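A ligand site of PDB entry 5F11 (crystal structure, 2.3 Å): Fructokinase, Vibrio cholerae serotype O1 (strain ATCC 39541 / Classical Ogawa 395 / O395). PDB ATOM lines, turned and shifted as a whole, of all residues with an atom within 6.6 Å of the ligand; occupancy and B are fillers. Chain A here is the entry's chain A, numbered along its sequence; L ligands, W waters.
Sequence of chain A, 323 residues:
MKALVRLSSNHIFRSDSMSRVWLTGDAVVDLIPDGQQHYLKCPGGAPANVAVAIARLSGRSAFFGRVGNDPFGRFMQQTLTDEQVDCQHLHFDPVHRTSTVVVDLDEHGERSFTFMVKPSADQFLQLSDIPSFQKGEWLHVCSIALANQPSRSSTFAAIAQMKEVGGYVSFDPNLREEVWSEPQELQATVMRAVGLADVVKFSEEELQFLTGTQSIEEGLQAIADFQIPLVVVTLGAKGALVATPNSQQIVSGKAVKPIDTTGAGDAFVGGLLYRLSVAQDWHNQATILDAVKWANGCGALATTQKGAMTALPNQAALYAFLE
O4 of the ligand sits at hydrogen-bond distance from ND2 of Asn 49. OD1 of Asp 30 is in hydrogen-bond range of O3 of the ligand (2.8 Å). O1 of the ligand is in hydrogen-bond range of N of Ala 46, 3.2 Å away. OD1 of Asp 26 sits at hydrogen-bond distance from O1 of the ligand. The backbone NH (N) of Gly 45 lies within hydrogen-bond range of an oxygen (O4) of the ligand. The side-chain carboxylate (OD2) of Asp 266 is in hydrogen-bond range of an oxygen (O6) of the ligand, at 2.7 Å. An oxygen (O6) of the ligand is in hydrogen-bond range of the guanidinium group (NH2) of Arg 176 (3.0 Å).
O of Val 29 is in hydrogen-bond range of N of Val 101. O of Gly 45 lies close to OD1 of Asn 49, at 3.2 Å. The backbone carbonyl oxygen (O) of Val 28 is in hydrogen-bond range of the backbone NH (N) of Gly 44 (2.8 Å). OD1 of Asn 174 is in hydrogen-bond range of NH2 of Arg 176 (3.2 Å). The side-chain amide nitrogen of Asn 49 lies within hydrogen-bond range of the side-chain carboxylate of Asp 266 (2.8 Å).
Val 28 touches the ligand. Gly 44 touches the ligand (CA to O4, 3.9 Å). Val 101 touches the ligand (CG2 to O3, 3.8 Å). Phe 113 touches the ligand (CG to O2, 3.5 Å). Phe 115 touches the ligand. Ile 144 touches the ligand. OD1 of Asn 174 touches O6 of the ligand, at 3.8 Å. Gly 263 touches the ligand. Hydrophobic or aromatic side chains within 4 Å of the ligand: Val 28, Ala 46, Val 101, Phe 113, Phe 115 and Ile 144. Of the 26 residues printed, 15 come within 4 Å of the ligand. The nearest printed residue that does not touch the ligand is Ala 308 (4.2 Å).
Water W1 lies within hydrogen-bond range of OD2 of Asp 26 (2.6 Å), O1 of the ligand (2.8 Å) and ND2 of Asn 174 (3.4 Å).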
ATOM      1  N   ASP A  26      28.833   4.011 -20.232  1.00  0.00           N
ATOM      2  CA  ASP A  26      30.108   3.353 -20.457  1.00  0.00           C
ATOM      3  C   ASP A  26      30.100   2.333 -21.598  1.00  0.00           C
ATOM      4  O   ASP A  26      29.283   1.420 -21.621  1.00  0.00           O
ATOM      5  CB  ASP A  26      30.633   2.725 -19.159  1.00  0.00           C
ATOM      6  CG  ASP A  26      29.739   1.632 -18.605  1.00  0.00           C
ATOM      7  OD1 ASP A  26      30.262   0.545 -18.296  1.00  0.00           O
ATOM      8  OD2 ASP A  26      28.514   1.851 -18.445  1.00  0.00           O
ATOM      9  N   ALA A  27      30.990   2.524 -22.573  1.00  0.00           N
ATOM     10  CA  ALA A  27      31.325   1.483 -23.556  1.00  0.00           C
ATOM     11  C   ALA A  27      32.627   0.865 -23.083  1.00  0.00           C
ATOM     12  O   ALA A  27      33.572   1.600 -22.799  1.00  0.00           O
ATOM     13  CB  ALA A  27      31.506   2.086 -24.939  1.00  0.00           C
ATOM     14  N   VAL A  28      32.677  -0.455 -22.956  1.00  0.00           N
ATOM     15  CA  VAL A  28      33.881  -1.070 -22.412  1.00  0.00           C
ATOM     16  C   VAL A  28      34.338  -2.327 -23.148  1.00  0.00           C
ATOM     17  O   VAL A  28      33.542  -3.051 -23.743  1.00  0.00           O
ATOM     18  CB  VAL A  28      33.789  -1.369 -20.875  1.00  0.00           C
ATOM     19  CG1 VAL A  28      32.654  -0.587 -20.211  1.00  0.00           C
ATOM     20  CG2 VAL A  28      33.654  -2.857 -20.604  1.00  0.00           C
ATOM     21  N   VAL A  29      35.645  -2.551 -23.124  1.00  0.00           N
ATOM     22  CA  VAL A  29      36.218  -3.772 -23.645  1.00  0.00           C
ATOM     23  C   VAL A  29      36.267  -4.800 -22.522  1.00  0.00           C
ATOM     24  O   VAL A  29      36.933  -4.590 -21.496  1.00  0.00           O
ATOM     25  CB  VAL A  29      37.625  -3.537 -24.215  1.00  0.00           C
ATOM     26  CG1 VAL A  29      38.215  -4.845 -24.707  1.00  0.00           C
ATOM     27  CG2 VAL A  29      37.562  -2.533 -25.337  1.00  0.00           C
ATOM     28  N   ASP A  30      35.550  -5.905 -22.729  1.00  0.00           N
ATOM     29  CA  ASP A  30      35.498  -7.007 -21.777  1.00  0.00           C
ATOM     30  C   ASP A  30      36.547  -8.073 -22.081  1.00  0.00           C
ATOM     31  O   ASP A  30      36.498  -8.738 -23.116  1.00  0.00           O
ATOM     32  CB  ASP A  30      34.117  -7.657 -21.800  1.00  0.00           C
ATOM     33  CG  ASP A  30      33.042  -6.768 -21.197  1.00  0.00           C
ATOM     34  OD1 ASP A  30      33.349  -5.995 -20.262  1.00  0.00           O
ATOM     35  OD2 ASP A  30      31.889  -6.855 -21.675  1.00  0.00           O
ATOM     36  N   PRO A  43      33.521  -6.734 -27.314  1.00  0.00           N
ATOM     37  CA  PRO A  43      32.869  -5.441 -27.110  1.00  0.00           C
ATOM     38  C   PRO A  43      31.853  -5.575 -25.981  1.00  0.00           C
ATOM     39  O   PRO A  43      31.292  -6.663 -25.763  1.00  0.00           O
ATOM     40  CB  PRO A  43      32.167  -5.198 -28.449  1.00  0.00           C
ATOM     41  CG  PRO A  43      31.909  -6.594 -28.983  1.00  0.00           C
ATOM     42  CD  PRO A  43      33.114  -7.390 -28.564  1.00  0.00           C
ATOM     43  N   GLY A  44      31.626  -4.493 -25.241  1.00  0.00           N
ATOM     44  CA  GLY A  44      30.772  -4.534 -24.070  1.00  0.00           C
ATOM     45  C   GLY A  44      30.436  -3.165 -23.501  1.00  0.00           C
ATOM     46  O   GLY A  44      30.488  -2.164 -24.224  1.00  0.00           O
ATOM     47  N   GLY A  45      30.106  -3.112 -22.225  1.00  0.00           N
ATOM     48  CA  GLY A  45      29.668  -1.869 -21.621  1.00  0.00           C
ATOM     49  C   GLY A  45      28.159  -1.864 -21.712  1.00  0.00           C
ATOM     50  O   GLY A  45      27.616  -1.889 -22.812  1.00  0.00           O
ATOM     51  N   ALA A  46      27.502  -1.853 -20.566  1.00  0.00           N
ATOM     52  CA  ALA A  46      26.057  -2.055 -20.501  1.00  0.00           C
ATOM     53  C   ALA A  46      25.222  -1.203 -21.458  1.00  0.00           C
ATOM     54  O   ALA A  46      24.420  -1.751 -22.212  1.00  0.00           O
ATOM     55  CB  ALA A  46      25.558  -1.929 -19.078  1.00  0.00           C
ATOM     56  N   PRO A  47      25.408   0.128 -21.463  1.00  0.00           N
ATOM     57  CA  PRO A  47      24.520   0.860 -22.375  1.00  0.00           C
ATOM     58  C   PRO A  47      24.879   0.613 -23.833  1.00  0.00           C
ATOM     59  O   PRO A  47      24.018   0.742 -24.709  1.00  0.00           O
ATOM     60  CB  PRO A  47      24.759   2.333 -21.992  1.00  0.00           C
ATOM     61  CG  PRO A  47      26.114   2.369 -21.387  1.00  0.00           C
ATOM     62  CD  PRO A  47      26.281   1.036 -20.687  1.00  0.00           C
ATOM     63  N   ASN A  49      25.669  -2.334 -24.852  1.00  0.00           N
ATOM     64  CA  ASN A  49      25.061  -3.624 -25.098  1.00  0.00           C
ATOM     65  C   ASN A  49      23.607  -3.466 -25.502  1.00  0.00           C
ATOM     66  O   ASN A  49      23.127  -4.082 -26.470  1.00  0.00           O
ATOM     67  CB  ASN A  49      25.152  -4.520 -23.864  1.00  0.00           C
ATOM     68  CG  ASN A  49      26.573  -4.830 -23.458  1.00  0.00           C
ATOM     69  OD1 ASN A  49      27.490  -4.759 -24.268  1.00  0.00           O
ATOM     70  ND2 ASN A  49      26.753  -5.206 -22.198  1.00  0.00           N
ATOM     71  N   SER A  99      37.211   2.362 -20.738  1.00  0.00           N
ATOM     72  CA  SER A  99      36.953   1.366 -19.693  1.00  0.00           C
ATOM     73  C   SER A  99      37.412  -0.035 -20.128  1.00  0.00           C
ATOM     74  O   SER A  99      37.228  -0.442 -21.286  1.00  0.00           O
ATOM     75  CB  SER A  99      35.468   1.377 -19.303  1.00  0.00           C
ATOM     76  OG  SER A  99      35.180   0.549 -18.190  1.00  0.00           O
ATOM     77  N   VAL A 101      37.509  -4.070 -18.546  1.00  0.00           N
ATOM     78  CA  VAL A 101      37.044  -4.941 -17.479  1.00  0.00           C
ATOM     79  C   VAL A 101      37.459  -6.402 -17.677  1.00  0.00           C
ATOM     80  O   VAL A 101      37.337  -6.966 -18.765  1.00  0.00           O
ATOM     81  CB  VAL A 101      35.504  -4.854 -17.297  1.00  0.00           C
ATOM     82  CG1 VAL A 101      35.055  -5.638 -16.062  1.00  0.00           C
ATOM     83  CG2 VAL A 101      35.053  -3.403 -17.161  1.00  0.00           C
ATOM     84  N   VAL A 103      36.719 -10.237 -16.757  1.00  0.00           N
ATOM     85  CA  VAL A 103      35.627 -11.091 -16.276  1.00  0.00           C
ATOM     86  C   VAL A 103      36.105 -12.378 -15.591  1.00  0.00           C
ATOM     87  O   VAL A 103      36.994 -13.073 -16.072  1.00  0.00           O
ATOM     88  CB  VAL A 103      34.637 -11.432 -17.419  1.00  0.00           C
ATOM     89  CG1 VAL A 103      33.438 -12.189 -16.869  1.00  0.00           C
ATOM     90  CG2 VAL A 103      34.174 -10.178 -18.108  1.00  0.00           C
ATOM     91  N   GLY A 109      26.955 -11.572 -12.682  1.00  0.00           N
ATOM     92  CA  GLY A 109      26.530 -10.225 -12.370  1.00  0.00           C
ATOM     93  C   GLY A 109      27.691  -9.401 -11.859  1.00  0.00           C
ATOM     94  O   GLY A 109      28.850  -9.681 -12.193  1.00  0.00           O
ATOM     95  N   PHE A 113      32.936  -8.857 -12.207  1.00  0.00           N
ATOM     96  CA  PHE A 113      33.723  -7.827 -12.871  1.00  0.00           C
ATOM     97  C   PHE A 113      34.851  -7.208 -12.036  1.00  0.00           C
ATOM     98  O   PHE A 113      34.713  -6.969 -10.836  1.00  0.00           O
ATOM     99  CB  PHE A 113      32.793  -6.747 -13.410  1.00  0.00           C
ATOM    100  CG  PHE A 113      31.732  -7.272 -14.323  1.00  0.00           C
ATOM    101  CD1 PHE A 113      30.419  -7.362 -13.899  1.00  0.00           C
ATOM    102  CD2 PHE A 113      32.057  -7.718 -15.585  1.00  0.00           C
ATOM    103  CE1 PHE A 113      29.437  -7.868 -14.745  1.00  0.00           C
ATOM    104  CE2 PHE A 113      31.075  -8.224 -16.431  1.00  0.00           C
ATOM    105  CZ  PHE A 113      29.769  -8.300 -16.009  1.00  0.00           C
ATOM    106  N   PHE A 115      37.122  -3.832 -12.534  1.00  0.00           N
ATOM    107  CA  PHE A 115      37.274  -2.618 -13.340  1.00  0.00           C
ATOM    108  C   PHE A 115      38.707  -2.091 -13.285  1.00  0.00           C
ATOM    109  O   PHE A 115      39.172  -1.710 -12.217  1.00  0.00           O
ATOM    110  CB  PHE A 115      36.277  -1.543 -12.893  1.00  0.00           C
ATOM    111  CG  PHE A 115      34.848  -1.856 -13.249  1.00  0.00           C
ATOM    112  CD1 PHE A 115      34.221  -1.207 -14.292  1.00  0.00           C
ATOM    113  CD2 PHE A 115      34.138  -2.811 -12.535  1.00  0.00           C
ATOM    114  CE1 PHE A 115      32.933  -1.507 -14.628  1.00  0.00           C
ATOM    115  CE2 PHE A 115      32.850  -3.118 -12.859  1.00  0.00           C
ATOM    116  CZ  PHE A 115      32.237  -2.461 -13.914  1.00  0.00           C
ATOM    117  N   ILE A 144      26.362   3.317 -13.566  1.00  0.00           N
ATOM    118  CA  ILE A 144      27.773   3.689 -13.759  1.00  0.00           C
ATOM    119  C   ILE A 144      27.862   5.133 -14.269  1.00  0.00           C
ATOM    120  O   ILE A 144      28.821   5.860 -13.990  1.00  0.00           O
ATOM    121  CB  ILE A 144      28.539   2.706 -14.696  1.00  0.00           C
ATOM    122  CG1 ILE A 144      28.820   1.386 -13.959  1.00  0.00           C
ATOM    123  CG2 ILE A 144      29.855   3.316 -15.155  1.00  0.00           C
ATOM    124  CD1 ILE A 144      29.681   0.413 -14.736  1.00  0.00           C
ATOM    125  N   ASN A 174      21.748  -1.660 -12.621  1.00  0.00           N
ATOM    126  CA  ASN A 174      22.905  -2.371 -13.170  1.00  0.00           C
ATOM    127  C   ASN A 174      24.174  -2.074 -12.358  1.00  0.00           C
ATOM    128  O   ASN A 174      25.157  -1.538 -12.892  1.00  0.00           O
ATOM    129  CB  ASN A 174      23.096  -1.992 -14.645  1.00  0.00           C
ATOM    130  CG  ASN A 174      24.077  -2.913 -15.371  1.00  0.00           C
ATOM    131  OD1 ASN A 174      23.829  -4.111 -15.532  1.00  0.00           O
ATOM    132  ND2 ASN A 174      25.189  -2.341 -15.807  1.00  0.00           N
ATOM    133  N   ARG A 176      27.494  -1.589 -10.189  1.00  0.00           N
ATOM    134  CA  ARG A 176      28.910  -1.968 -10.137  1.00  0.00           C
ATOM    135  C   ARG A 176      29.618  -1.047  -9.151  1.00  0.00           C
ATOM    136  O   ARG A 176      30.177  -0.004  -9.527  1.00  0.00           O
ATOM    137  CB  ARG A 176      29.582  -1.853 -11.513  1.00  0.00           C
ATOM    138  CG  ARG A 176      28.839  -2.540 -12.639  1.00  0.00           C
ATOM    139  CD  ARG A 176      28.948  -4.056 -12.613  1.00  0.00           C
ATOM    140  NE  ARG A 176      28.405  -4.595 -13.847  1.00  0.00           N
ATOM    141  CZ  ARG A 176      27.144  -5.015 -14.000  1.00  0.00           C
ATOM    142  NH1 ARG A 176      26.308  -4.997 -12.968  1.00  0.00           N
ATOM    143  NH2 ARG A 176      26.735  -5.454 -15.186  1.00  0.00           N
ATOM    144  N   THR A 262      27.090 -13.058 -19.083  1.00  0.00           N
ATOM    145  CA  THR A 262      27.511 -11.673 -19.293  1.00  0.00           C
ATOM    146  C   THR A 262      26.600 -10.839 -20.201  1.00  0.00           C
ATOM    147  O   THR A 262      26.422 -11.161 -21.383  1.00  0.00           O
ATOM    148  CB  THR A 262      28.957 -11.610 -19.827  1.00  0.00           C
ATOM    149  OG1 THR A 262      29.823 -12.307 -18.935  1.00  0.00           O
ATOM    150  CG2 THR A 262      29.420 -10.153 -19.962  1.00  0.00           C
ATOM    151  N   GLY A 263      26.016  -9.779 -19.643  1.00  0.00           N
ATOM    152  CA  GLY A 263      25.205  -8.849 -20.399  1.00  0.00           C
ATOM    153  C   GLY A 263      23.809  -9.347 -20.717  1.00  0.00           C
ATOM    154  O   GLY A 263      23.088  -8.737 -21.518  1.00  0.00           O
ATOM    155  N   ALA A 264      23.433 -10.460 -20.083  1.00  0.00           N
ATOM    156  CA  ALA A 264      22.104 -11.039 -20.263  1.00  0.00           C
ATOM    157  C   ALA A 264      21.009 -10.047 -19.895  1.00  0.00           C
ATOM    158  O   ALA A 264      20.036  -9.877 -20.645  1.00  0.00           O
ATOM    159  CB  ALA A 264      21.961 -12.312 -19.436  1.00  0.00           C
ATOM    160  N   GLY A 265      21.152  -9.407 -18.738  1.00  0.00           N
ATOM    161  CA  GLY A 265      20.233  -8.362 -18.318  1.00  0.00           C
ATOM    162  C   GLY A 265      20.106  -7.215 -19.328  1.00  0.00           C
ATOM    163  O   GLY A 265      19.052  -6.613 -19.456  1.00  0.00           O
ATOM    164  N   ASP A 266      21.191  -6.921 -20.042  1.00  0.00           N
ATOM    165  CA  ASP A 266      21.158  -5.857 -21.030  1.00  0.00           C
ATOM    166  C   ASP A 266      20.336  -6.275 -22.257  1.00  0.00           C
ATOM    167  O   ASP A 266      19.616  -5.451 -22.831  1.00  0.00           O
ATOM    168  CB  ASP A 266      22.585  -5.449 -21.440  1.00  0.00           C
ATOM    169  CG  ASP A 266      23.433  -5.017 -20.255  1.00  0.00           C
ATOM    170  OD1 ASP A 266      22.854  -4.514 -19.272  1.00  0.00           O
ATOM    171  OD2 ASP A 266      24.667  -5.190 -20.298  1.00  0.00           O
ATOM    172  N   ALA A 308      29.028 -10.130 -24.232  1.00  0.00           N
ATOM    173  CA  ALA A 308      27.724  -9.503 -24.074  1.00  0.00           C
ATOM    174  C   ALA A 308      26.953  -9.357 -25.387  1.00  0.00           C
ATOM    175  O   ALA A 308      25.740  -9.534 -25.422  1.00  0.00           O
ATOM    176  CB  ALA A 308      27.865  -8.127 -23.392  1.00  0.00           C
HETATM  177  C1  LIG L   1      29.882  -2.564 -17.005  1.00  0.00           C
HETATM  178  C2  LIG L   1      29.700  -4.022 -17.315  1.00  0.00           C
HETATM  179  C3  LIG L   1      30.376  -4.355 -18.603  1.00  0.00           C
HETATM  180  C4  LIG L   1      29.547  -5.465 -19.097  1.00  0.00           C
HETATM  181  C5  LIG L   1      28.200  -4.965 -18.726  1.00  0.00           C
HETATM  182  C6  LIG L   1      27.263  -6.136 -18.669  1.00  0.00           C
HETATM  183  O1  LIG L   1      29.282  -1.760 -17.957  1.00  0.00           O
HETATM  184  O2  LIG L   1      30.230  -4.721 -16.249  1.00  0.00           O
HETATM  185  O3  LIG L   1      31.681  -4.744 -18.439  1.00  0.00           O
HETATM  186  O4  LIG L   1      29.646  -5.648 -20.452  1.00  0.00           O
HETATM  187  O5  LIG L   1      28.338  -4.331 -17.481  1.00  0.00           O
HETATM  188  O6  LIG L   1      26.072  -5.814 -18.054  1.00  0.00           O
HETATM  189  O   HOH W   1      27.225  -0.012 -17.151  1.00  0.00           O
